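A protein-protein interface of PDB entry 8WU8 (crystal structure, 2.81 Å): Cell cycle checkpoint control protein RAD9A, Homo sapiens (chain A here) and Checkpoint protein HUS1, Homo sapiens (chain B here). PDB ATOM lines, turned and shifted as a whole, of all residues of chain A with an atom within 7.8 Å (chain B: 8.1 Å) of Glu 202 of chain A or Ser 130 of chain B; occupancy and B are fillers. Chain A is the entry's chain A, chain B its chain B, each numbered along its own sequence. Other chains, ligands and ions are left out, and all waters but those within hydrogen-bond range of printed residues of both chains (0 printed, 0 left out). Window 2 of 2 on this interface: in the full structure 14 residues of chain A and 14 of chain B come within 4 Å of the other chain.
NE of Arg 133 of chain B lies within salt-bridge range of OD2 of Asp 203 of chain A (2.8 Å).
Of the 8 printed residues of chain B, 3 touch a printed residue of chain A.
Printed residues of chain A that touch a printed residue of chain B: Leu 199, Gly 200, Glu 202 and Asp 203.
Hydrophobic or aromatic side chains of chain A within 4 Å of the printed part of chain B: Leu 199.
Among the printed residues, 5 pairs touch across the chains.
Among the printed residues, Asp or Glu carboxylates within 4 Å of a Lys or Arg side-chain nitrogen of the other chain: Asp 203 of chain A with Arg 133 of chain B (2.8 Å).
Among the printed residues, merely in contact across the chains: Leu 199 of chain A with Arg 133 of chain B (3.5 Å), Gly 200 of chain A with Ser 131 of chain B (3.9 Å), Glu 202 of chain A with Ser 130 of chain B (3.5 Å) and Glu 202 of chain A with Ser 131 of chain B (3.7 Å).
Arg 146 of chain A touches none of the printed residues of chain B.
Printed residues of chain B within 4 Å of Leu 199 of chain A: Arg 133 (3.5 Å).
Of chain B, only Ser 130 and Ser 131 come within 4 Å of Glu 202 of chain A.
Of chain A, only Glu 202 (3.5 Å) comes within 4 Å of Ser 130 of chain B.
Printed residues of chain A within 4 Å of Ser 131 of chain B: Gly 200 (3.9 Å) and Glu 202 (3.7 Å).
Ser 132 of chain B touches none of the printed residues of chain A.
Of the printed residues of chain A, Arg 133 of chain B touches Leu 199 (3.5 Å) and Asp 203 (2.8 Å).
The nearest residue of chain B that does not touch Glu 202 of chain A is Ser 129 of chain B (5.9 Å).
The nearest residue of chain A that does not touch Ser 130 of chain B is Asp 203 of chain A (4.7 Å).
The nearest printed residue of chain B that does not touch Asp 203 of chain A is Ser 130 of chain B (4.7 Å).
The backbone carbonyl oxygen of Val 176 of chain A is in hydrogen-bond range of the backbone NH of Leu 199 of chain A (2.7 Å).
The side-chain hydroxyl (OG) of Ser 127 of chain B lies within hydrogen-bond range of the backbone carbonyl oxygen (O) of Ser 131 of chain B.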
ATOM      1  N   ARG A 146       3.152  21.356  35.227  1.00  0.00           N
ATOM      2  CA  ARG A 146       1.755  21.561  34.875  1.00  0.00           C
ATOM      3  C   ARG A 146       1.625  22.621  33.786  1.00  0.00           C
ATOM      4  O   ARG A 146       2.181  23.712  33.900  1.00  0.00           O
ATOM      5  CB  ARG A 146       0.939  21.958  36.106  1.00  0.00           C
ATOM      6  CG  ARG A 146      -0.523  21.540  36.039  1.00  0.00           C
ATOM      7  CD  ARG A 146      -1.334  22.145  37.176  1.00  0.00           C
ATOM      8  NE  ARG A 146      -1.772  23.504  36.866  1.00  0.00           N
ATOM      9  CZ  ARG A 146      -2.258  24.357  37.763  1.00  0.00           C
ATOM     10  NH1 ARG A 146      -2.363  23.997  39.034  1.00  0.00           N
ATOM     11  NH2 ARG A 146      -2.633  25.573  37.389  1.00  0.00           N
ATOM     12  N   GLY A 173      18.473  27.684  34.844  1.00  0.00           N
ATOM     13  CA  GLY A 173      17.671  28.837  34.482  1.00  0.00           C
ATOM     14  C   GLY A 173      16.197  28.496  34.390  1.00  0.00           C
ATOM     15  O   GLY A 173      15.426  29.212  33.748  1.00  0.00           O
ATOM     16  N   ARG A 174      15.815  27.398  35.039  1.00  0.00           N
ATOM     17  CA  ARG A 174      14.437  26.914  35.036  1.00  0.00           C
ATOM     18  C   ARG A 174      13.910  26.718  33.616  1.00  0.00           C
ATOM     19  O   ARG A 174      12.822  27.181  33.271  1.00  0.00           O
ATOM     20  CB  ARG A 174      13.534  27.869  35.819  1.00  0.00           C
ATOM     21  CG  ARG A 174      13.909  27.990  37.286  1.00  0.00           C
ATOM     22  CD  ARG A 174      12.963  28.909  38.032  1.00  0.00           C
ATOM     23  NE  ARG A 174      13.362  29.078  39.428  1.00  0.00           N
ATOM     24  CZ  ARG A 174      12.722  29.853  40.298  1.00  0.00           C
ATOM     25  NH1 ARG A 174      11.649  30.534  39.920  1.00  0.00           N
ATOM     26  NH2 ARG A 174      13.156  29.947  41.548  1.00  0.00           N
ATOM     27  N   ARG A 175      14.703  26.036  32.797  1.00  0.00           N
ATOM     28  CA  ARG A 175      14.277  25.648  31.462  1.00  0.00           C
ATOM     29  C   ARG A 175      13.769  24.212  31.485  1.00  0.00           C
ATOM     30  O   ARG A 175      14.368  23.348  32.126  1.00  0.00           O
ATOM     31  CB  ARG A 175      15.426  25.770  30.456  1.00  0.00           C
ATOM     32  CG  ARG A 175      16.178  27.090  30.483  1.00  0.00           C
ATOM     33  CD  ARG A 175      15.293  28.252  30.082  1.00  0.00           C
ATOM     34  NE  ARG A 175      16.078  29.355  29.534  1.00  0.00           N
ATOM     35  CZ  ARG A 175      16.729  30.250  30.270  1.00  0.00           C
ATOM     36  NH1 ARG A 175      16.695  30.174  31.593  1.00  0.00           N
ATOM     37  NH2 ARG A 175      17.419  31.219  29.681  1.00  0.00           N
ATOM     38  N   VAL A 176      12.665  23.955  30.796  1.00  0.00           N
ATOM     39  CA  VAL A 176      12.220  22.584  30.593  1.00  0.00           C
ATOM     40  C   VAL A 176      12.778  22.074  29.274  1.00  0.00           C
ATOM     41  O   VAL A 176      12.464  22.608  28.214  1.00  0.00           O
ATOM     42  CB  VAL A 176      10.690  22.468  30.589  1.00  0.00           C
ATOM     43  CG1 VAL A 176      10.271  21.089  30.111  1.00  0.00           C
ATOM     44  CG2 VAL A 176      10.135  22.753  31.975  1.00  0.00           C
ATOM     45  N   LEU A 199      11.866  24.688  26.610  1.00  0.00           N
ATOM     46  CA  LEU A 199      10.815  25.593  27.071  1.00  0.00           C
ATOM     47  C   LEU A 199      11.336  26.510  28.174  1.00  0.00           C
ATOM     48  O   LEU A 199      12.317  26.191  28.846  1.00  0.00           O
ATOM     49  CB  LEU A 199       9.605  24.808  27.594  1.00  0.00           C
ATOM     50  CG  LEU A 199       8.833  23.839  26.693  1.00  0.00           C
ATOM     51  CD1 LEU A 199       8.608  24.450  25.330  1.00  0.00           C
ATOM     52  CD2 LEU A 199       9.517  22.477  26.581  1.00  0.00           C
ATOM     53  N   GLY A 200      10.680  27.650  28.356  1.00  0.00           N
ATOM     54  CA  GLY A 200      10.949  28.509  29.494  1.00  0.00           C
ATOM     55  C   GLY A 200       9.928  28.208  30.574  1.00  0.00           C
ATOM     56  O   GLY A 200       8.927  27.546  30.304  1.00  0.00           O
ATOM     57  N   GLU A 201      10.161  28.683  31.791  1.00  0.00           N
ATOM     58  CA  GLU A 201       9.232  28.398  32.881  1.00  0.00           C
ATOM     59  C   GLU A 201       7.975  29.256  32.788  1.00  0.00           C
ATOM     60  O   GLU A 201       7.014  29.046  33.529  1.00  0.00           O
ATOM     61  CB  GLU A 201       9.901  28.617  34.236  1.00  0.00           C
ATOM     62  CG  GLU A 201      10.215  30.070  34.538  1.00  0.00           C
ATOM     63  CD  GLU A 201      10.382  30.333  36.020  1.00  0.00           C
ATOM     64  OE1 GLU A 201      10.909  31.409  36.378  1.00  0.00           O
ATOM     65  OE2 GLU A 201       9.980  29.466  36.827  1.00  0.00           O
ATOM     66  N   GLU A 202       7.986  30.222  31.874  1.00  0.00           N
ATOM     67  CA  GLU A 202       6.893  31.178  31.757  1.00  0.00           C
ATOM     68  C   GLU A 202       5.588  30.546  31.278  1.00  0.00           C
ATOM     69  O   GLU A 202       4.540  30.736  31.896  1.00  0.00           O
ATOM     70  CB  GLU A 202       7.285  32.319  30.819  1.00  0.00           C
ATOM     71  CG  GLU A 202       8.014  33.474  31.492  1.00  0.00           C
ATOM     72  CD  GLU A 202       9.521  33.327  31.456  1.00  0.00           C
ATOM     73  OE1 GLU A 202      10.217  34.284  31.856  1.00  0.00           O
ATOM     74  OE2 GLU A 202      10.010  32.261  31.026  1.00  0.00           O
ATOM     75  N   ASP A 203       5.642  29.794  30.182  1.00  0.00           N
ATOM     76  CA  ASP A 203       4.438  29.154  29.656  1.00  0.00           C
ATOM     77  C   ASP A 203       4.085  27.890  30.444  1.00  0.00           C
ATOM     78  O   ASP A 203       3.358  27.023  29.961  1.00  0.00           O
ATOM     79  CB  ASP A 203       4.597  28.831  28.164  1.00  0.00           C
ATOM     80  CG  ASP A 203       5.957  28.250  27.831  1.00  0.00           C
ATOM     81  OD1 ASP A 203       6.643  27.765  28.754  1.00  0.00           O
ATOM     82  OD2 ASP A 203       6.337  28.271  26.641  1.00  0.00           O
ATOM     83  N   PHE A 204       4.611  27.802  31.662  1.00  0.00           N
ATOM     84  CA  PHE A 204       4.255  26.746  32.602  1.00  0.00           C
ATOM     85  C   PHE A 204       3.443  27.321  33.759  1.00  0.00           C
ATOM     86  O   PHE A 204       3.857  28.290  34.400  1.00  0.00           O
ATOM     87  CB  PHE A 204       5.509  26.048  33.136  1.00  0.00           C
ATOM     88  CG  PHE A 204       5.908  24.828  32.354  1.00  0.00           C
ATOM     89  CD1 PHE A 204       6.642  24.945  31.185  1.00  0.00           C
ATOM     90  CD2 PHE A 204       5.556  23.564  32.795  1.00  0.00           C
ATOM     91  CE1 PHE A 204       7.009  23.825  30.466  1.00  0.00           C
ATOM     92  CE2 PHE A 204       5.921  22.441  32.081  1.00  0.00           C
ATOM     93  CZ  PHE A 204       6.649  22.571  30.916  1.00  0.00           C
ATOM     94  N   GLN A 205       2.281  26.728  34.015  1.00  0.00           N
ATOM     95  CA  GLN A 205       1.432  27.147  35.123  1.00  0.00           C
ATOM     96  C   GLN A 205       2.100  26.831  36.459  1.00  0.00           C
ATOM     97  O   GLN A 205       2.128  27.660  37.370  1.00  0.00           O
ATOM     98  CB  GLN A 205       0.065  26.464  35.036  1.00  0.00           C
ATOM     99  CG  GLN A 205      -0.699  26.755  33.752  1.00  0.00           C
ATOM    100  CD  GLN A 205      -1.879  25.821  33.549  1.00  0.00           C
ATOM    101  OE1 GLN A 205      -1.940  24.744  34.140  1.00  0.00           O
ATOM    102  NE2 GLN A 205      -2.822  26.233  32.709  1.00  0.00           N
ATOM    103  N   GLN A 206       2.641  25.622  36.559  1.00  0.00           N
ATOM    104  CA  GLN A 206       3.340  25.174  37.756  1.00  0.00           C
ATOM    105  C   GLN A 206       4.646  24.488  37.383  1.00  0.00           C
ATOM    106  O   GLN A 206       4.694  23.704  36.436  1.00  0.00           O
ATOM    107  CB  GLN A 206       2.465  24.220  38.568  1.00  0.00           C
ATOM    108  CG  GLN A 206       1.923  24.795  39.860  1.00  0.00           C
ATOM    109  CD  GLN A 206       0.873  23.899  40.485  1.00  0.00           C
ATOM    110  OE1 GLN A 206       0.107  23.239  39.782  1.00  0.00           O
ATOM    111  NE2 GLN A 206       0.837  23.861  41.813  1.00  0.00           N
ATOM    112  N   LEU A 207       5.705  24.788  38.123  1.00  0.00           N
ATOM    113  CA  LEU A 207       6.995  24.153  37.892  1.00  0.00           C
ATOM    114  C   LEU A 207       7.751  24.033  39.202  1.00  0.00           C
ATOM    115  O   LEU A 207       8.363  24.995  39.663  1.00  0.00           O
ATOM    116  CB  LEU A 207       7.818  24.941  36.869  1.00  0.00           C
ATOM    117  CG  LEU A 207       8.936  24.198  36.128  1.00  0.00           C
ATOM    118  CD1 LEU A 207       9.279  24.921  34.837  1.00  0.00           C
ATOM    119  CD2 LEU A 207      10.186  24.036  36.982  1.00  0.00           C
ATOM    120  N   ARG B 105      10.260  32.022  13.554  1.00  0.00           N
ATOM    121  CA  ARG B 105      10.715  33.407  13.489  1.00  0.00           C
ATOM    122  C   ARG B 105      12.148  33.486  12.974  1.00  0.00           C
ATOM    123  O   ARG B 105      12.522  34.433  12.281  1.00  0.00           O
ATOM    124  CB  ARG B 105      10.630  34.075  14.869  1.00  0.00           C
ATOM    125  CG  ARG B 105       9.218  34.225  15.433  1.00  0.00           C
ATOM    126  CD  ARG B 105       9.224  34.932  16.788  1.00  0.00           C
ATOM    127  NE  ARG B 105       7.879  35.090  17.343  1.00  0.00           N
ATOM    128  CZ  ARG B 105       7.607  35.644  18.521  1.00  0.00           C
ATOM    129  NH1 ARG B 105       8.587  36.101  19.285  1.00  0.00           N
ATOM    130  NH2 ARG B 105       6.351  35.740  18.936  1.00  0.00           N
ATOM    131  N   SER B 127       6.790  32.289  19.465  1.00  0.00           N
ATOM    132  CA  SER B 127       6.583  32.412  20.870  1.00  0.00           C
ATOM    133  C   SER B 127       5.109  32.605  20.948  1.00  0.00           C
ATOM    134  O   SER B 127       4.575  33.614  20.521  1.00  0.00           O
ATOM    135  CB  SER B 127       7.317  33.624  21.427  1.00  0.00           C
ATOM    136  OG  SER B 127       7.301  33.615  22.842  1.00  0.00           O
ATOM    137  N   MET B 128       4.441  31.633  21.539  1.00  0.00           N
ATOM    138  CA  MET B 128       3.010  31.675  21.710  1.00  0.00           C
ATOM    139  C   MET B 128       2.814  32.882  22.578  1.00  0.00           C
ATOM    140  O   MET B 128       1.896  33.661  22.447  1.00  0.00           O
ATOM    141  CB  MET B 128       2.577  30.424  22.463  1.00  0.00           C
ATOM    142  CG  MET B 128       2.350  29.210  21.584  1.00  0.00           C
ATOM    143  SD  MET B 128       0.951  29.360  20.465  1.00  0.00           S
ATOM    144  CE  MET B 128       0.232  30.936  20.931  1.00  0.00           C
ATOM    145  N   SER B 129       3.756  32.993  23.480  1.00  0.00           N
ATOM    146  CA  SER B 129       3.918  34.181  24.305  1.00  0.00           C
ATOM    147  C   SER B 129       5.164  34.023  25.161  1.00  0.00           C
ATOM    148  O   SER B 129       5.829  32.987  25.114  1.00  0.00           O
ATOM    149  CB  SER B 129       2.695  34.418  25.197  1.00  0.00           C
ATOM    150  OG  SER B 129       1.575  34.835  24.436  1.00  0.00           O
ATOM    151  N   SER B 130       5.476  35.065  25.925  1.00  0.00           N
ATOM    152  CA  SER B 130       6.474  34.987  26.984  1.00  0.00           C
ATOM    153  C   SER B 130       7.880  34.673  26.478  1.00  0.00           C
ATOM    154  O   SER B 130       8.600  35.563  26.021  1.00  0.00           O
ATOM    155  CB  SER B 130       6.050  33.937  28.012  1.00  0.00           C
ATOM    156  OG  SER B 130       4.682  34.075  28.351  1.00  0.00           O
ATOM    157  N   SER B 131       8.265  33.403  26.569  1.00  0.00           N
ATOM    158  CA  SER B 131       9.630  32.990  26.262  1.00  0.00           C
ATOM    159  C   SER B 131       9.778  32.397  24.865  1.00  0.00           C
ATOM    160  O   SER B 131       8.792  32.107  24.186  1.00  0.00           O
ATOM    161  CB  SER B 131      10.118  31.977  27.297  1.00  0.00           C
ATOM    162  OG  SER B 131      11.386  31.455  26.937  1.00  0.00           O
ATOM    163  N   SER B 132      11.026  32.216  24.449  1.00  0.00           N
ATOM    164  CA  SER B 132      11.326  31.639  23.147  1.00  0.00           C
ATOM    165  C   SER B 132      11.369  30.118  23.220  1.00  0.00           C
ATOM    166  O   SER B 132      12.018  29.545  24.095  1.00  0.00           O
ATOM    167  CB  SER B 132      12.655  32.174  22.613  1.00  0.00           C
ATOM    168  OG  SER B 132      12.650  33.589  22.553  1.00  0.00           O
ATOM    169  N   ARG B 133      10.659  29.471  22.303  1.00  0.00           N
ATOM    170  CA  ARG B 133      10.738  28.026  22.153  1.00  0.00           C
ATOM    171  C   ARG B 133      11.889  27.705  21.209  1.00  0.00           C
ATOM    172  O   ARG B 133      11.847  28.067  20.034  1.00  0.00           O
ATOM    173  CB  ARG B 133       9.429  27.454  21.610  1.00  0.00           C
ATOM    174  CG  ARG B 133       8.173  28.062  22.207  1.00  0.00           C
ATOM    175  CD  ARG B 133       7.773  27.365  23.491  1.00  0.00           C
ATOM    176  NE  ARG B 133       6.423  27.732  23.901  1.00  0.00           N
ATOM    177  CZ  ARG B 133       5.318  27.222  23.366  1.00  0.00           C
ATOM    178  NH1 ARG B 133       5.402  26.320  22.397  1.00  0.00           N
ATOM    179  NH2 ARG B 133       4.128  27.614  23.799  1.00  0.00           N
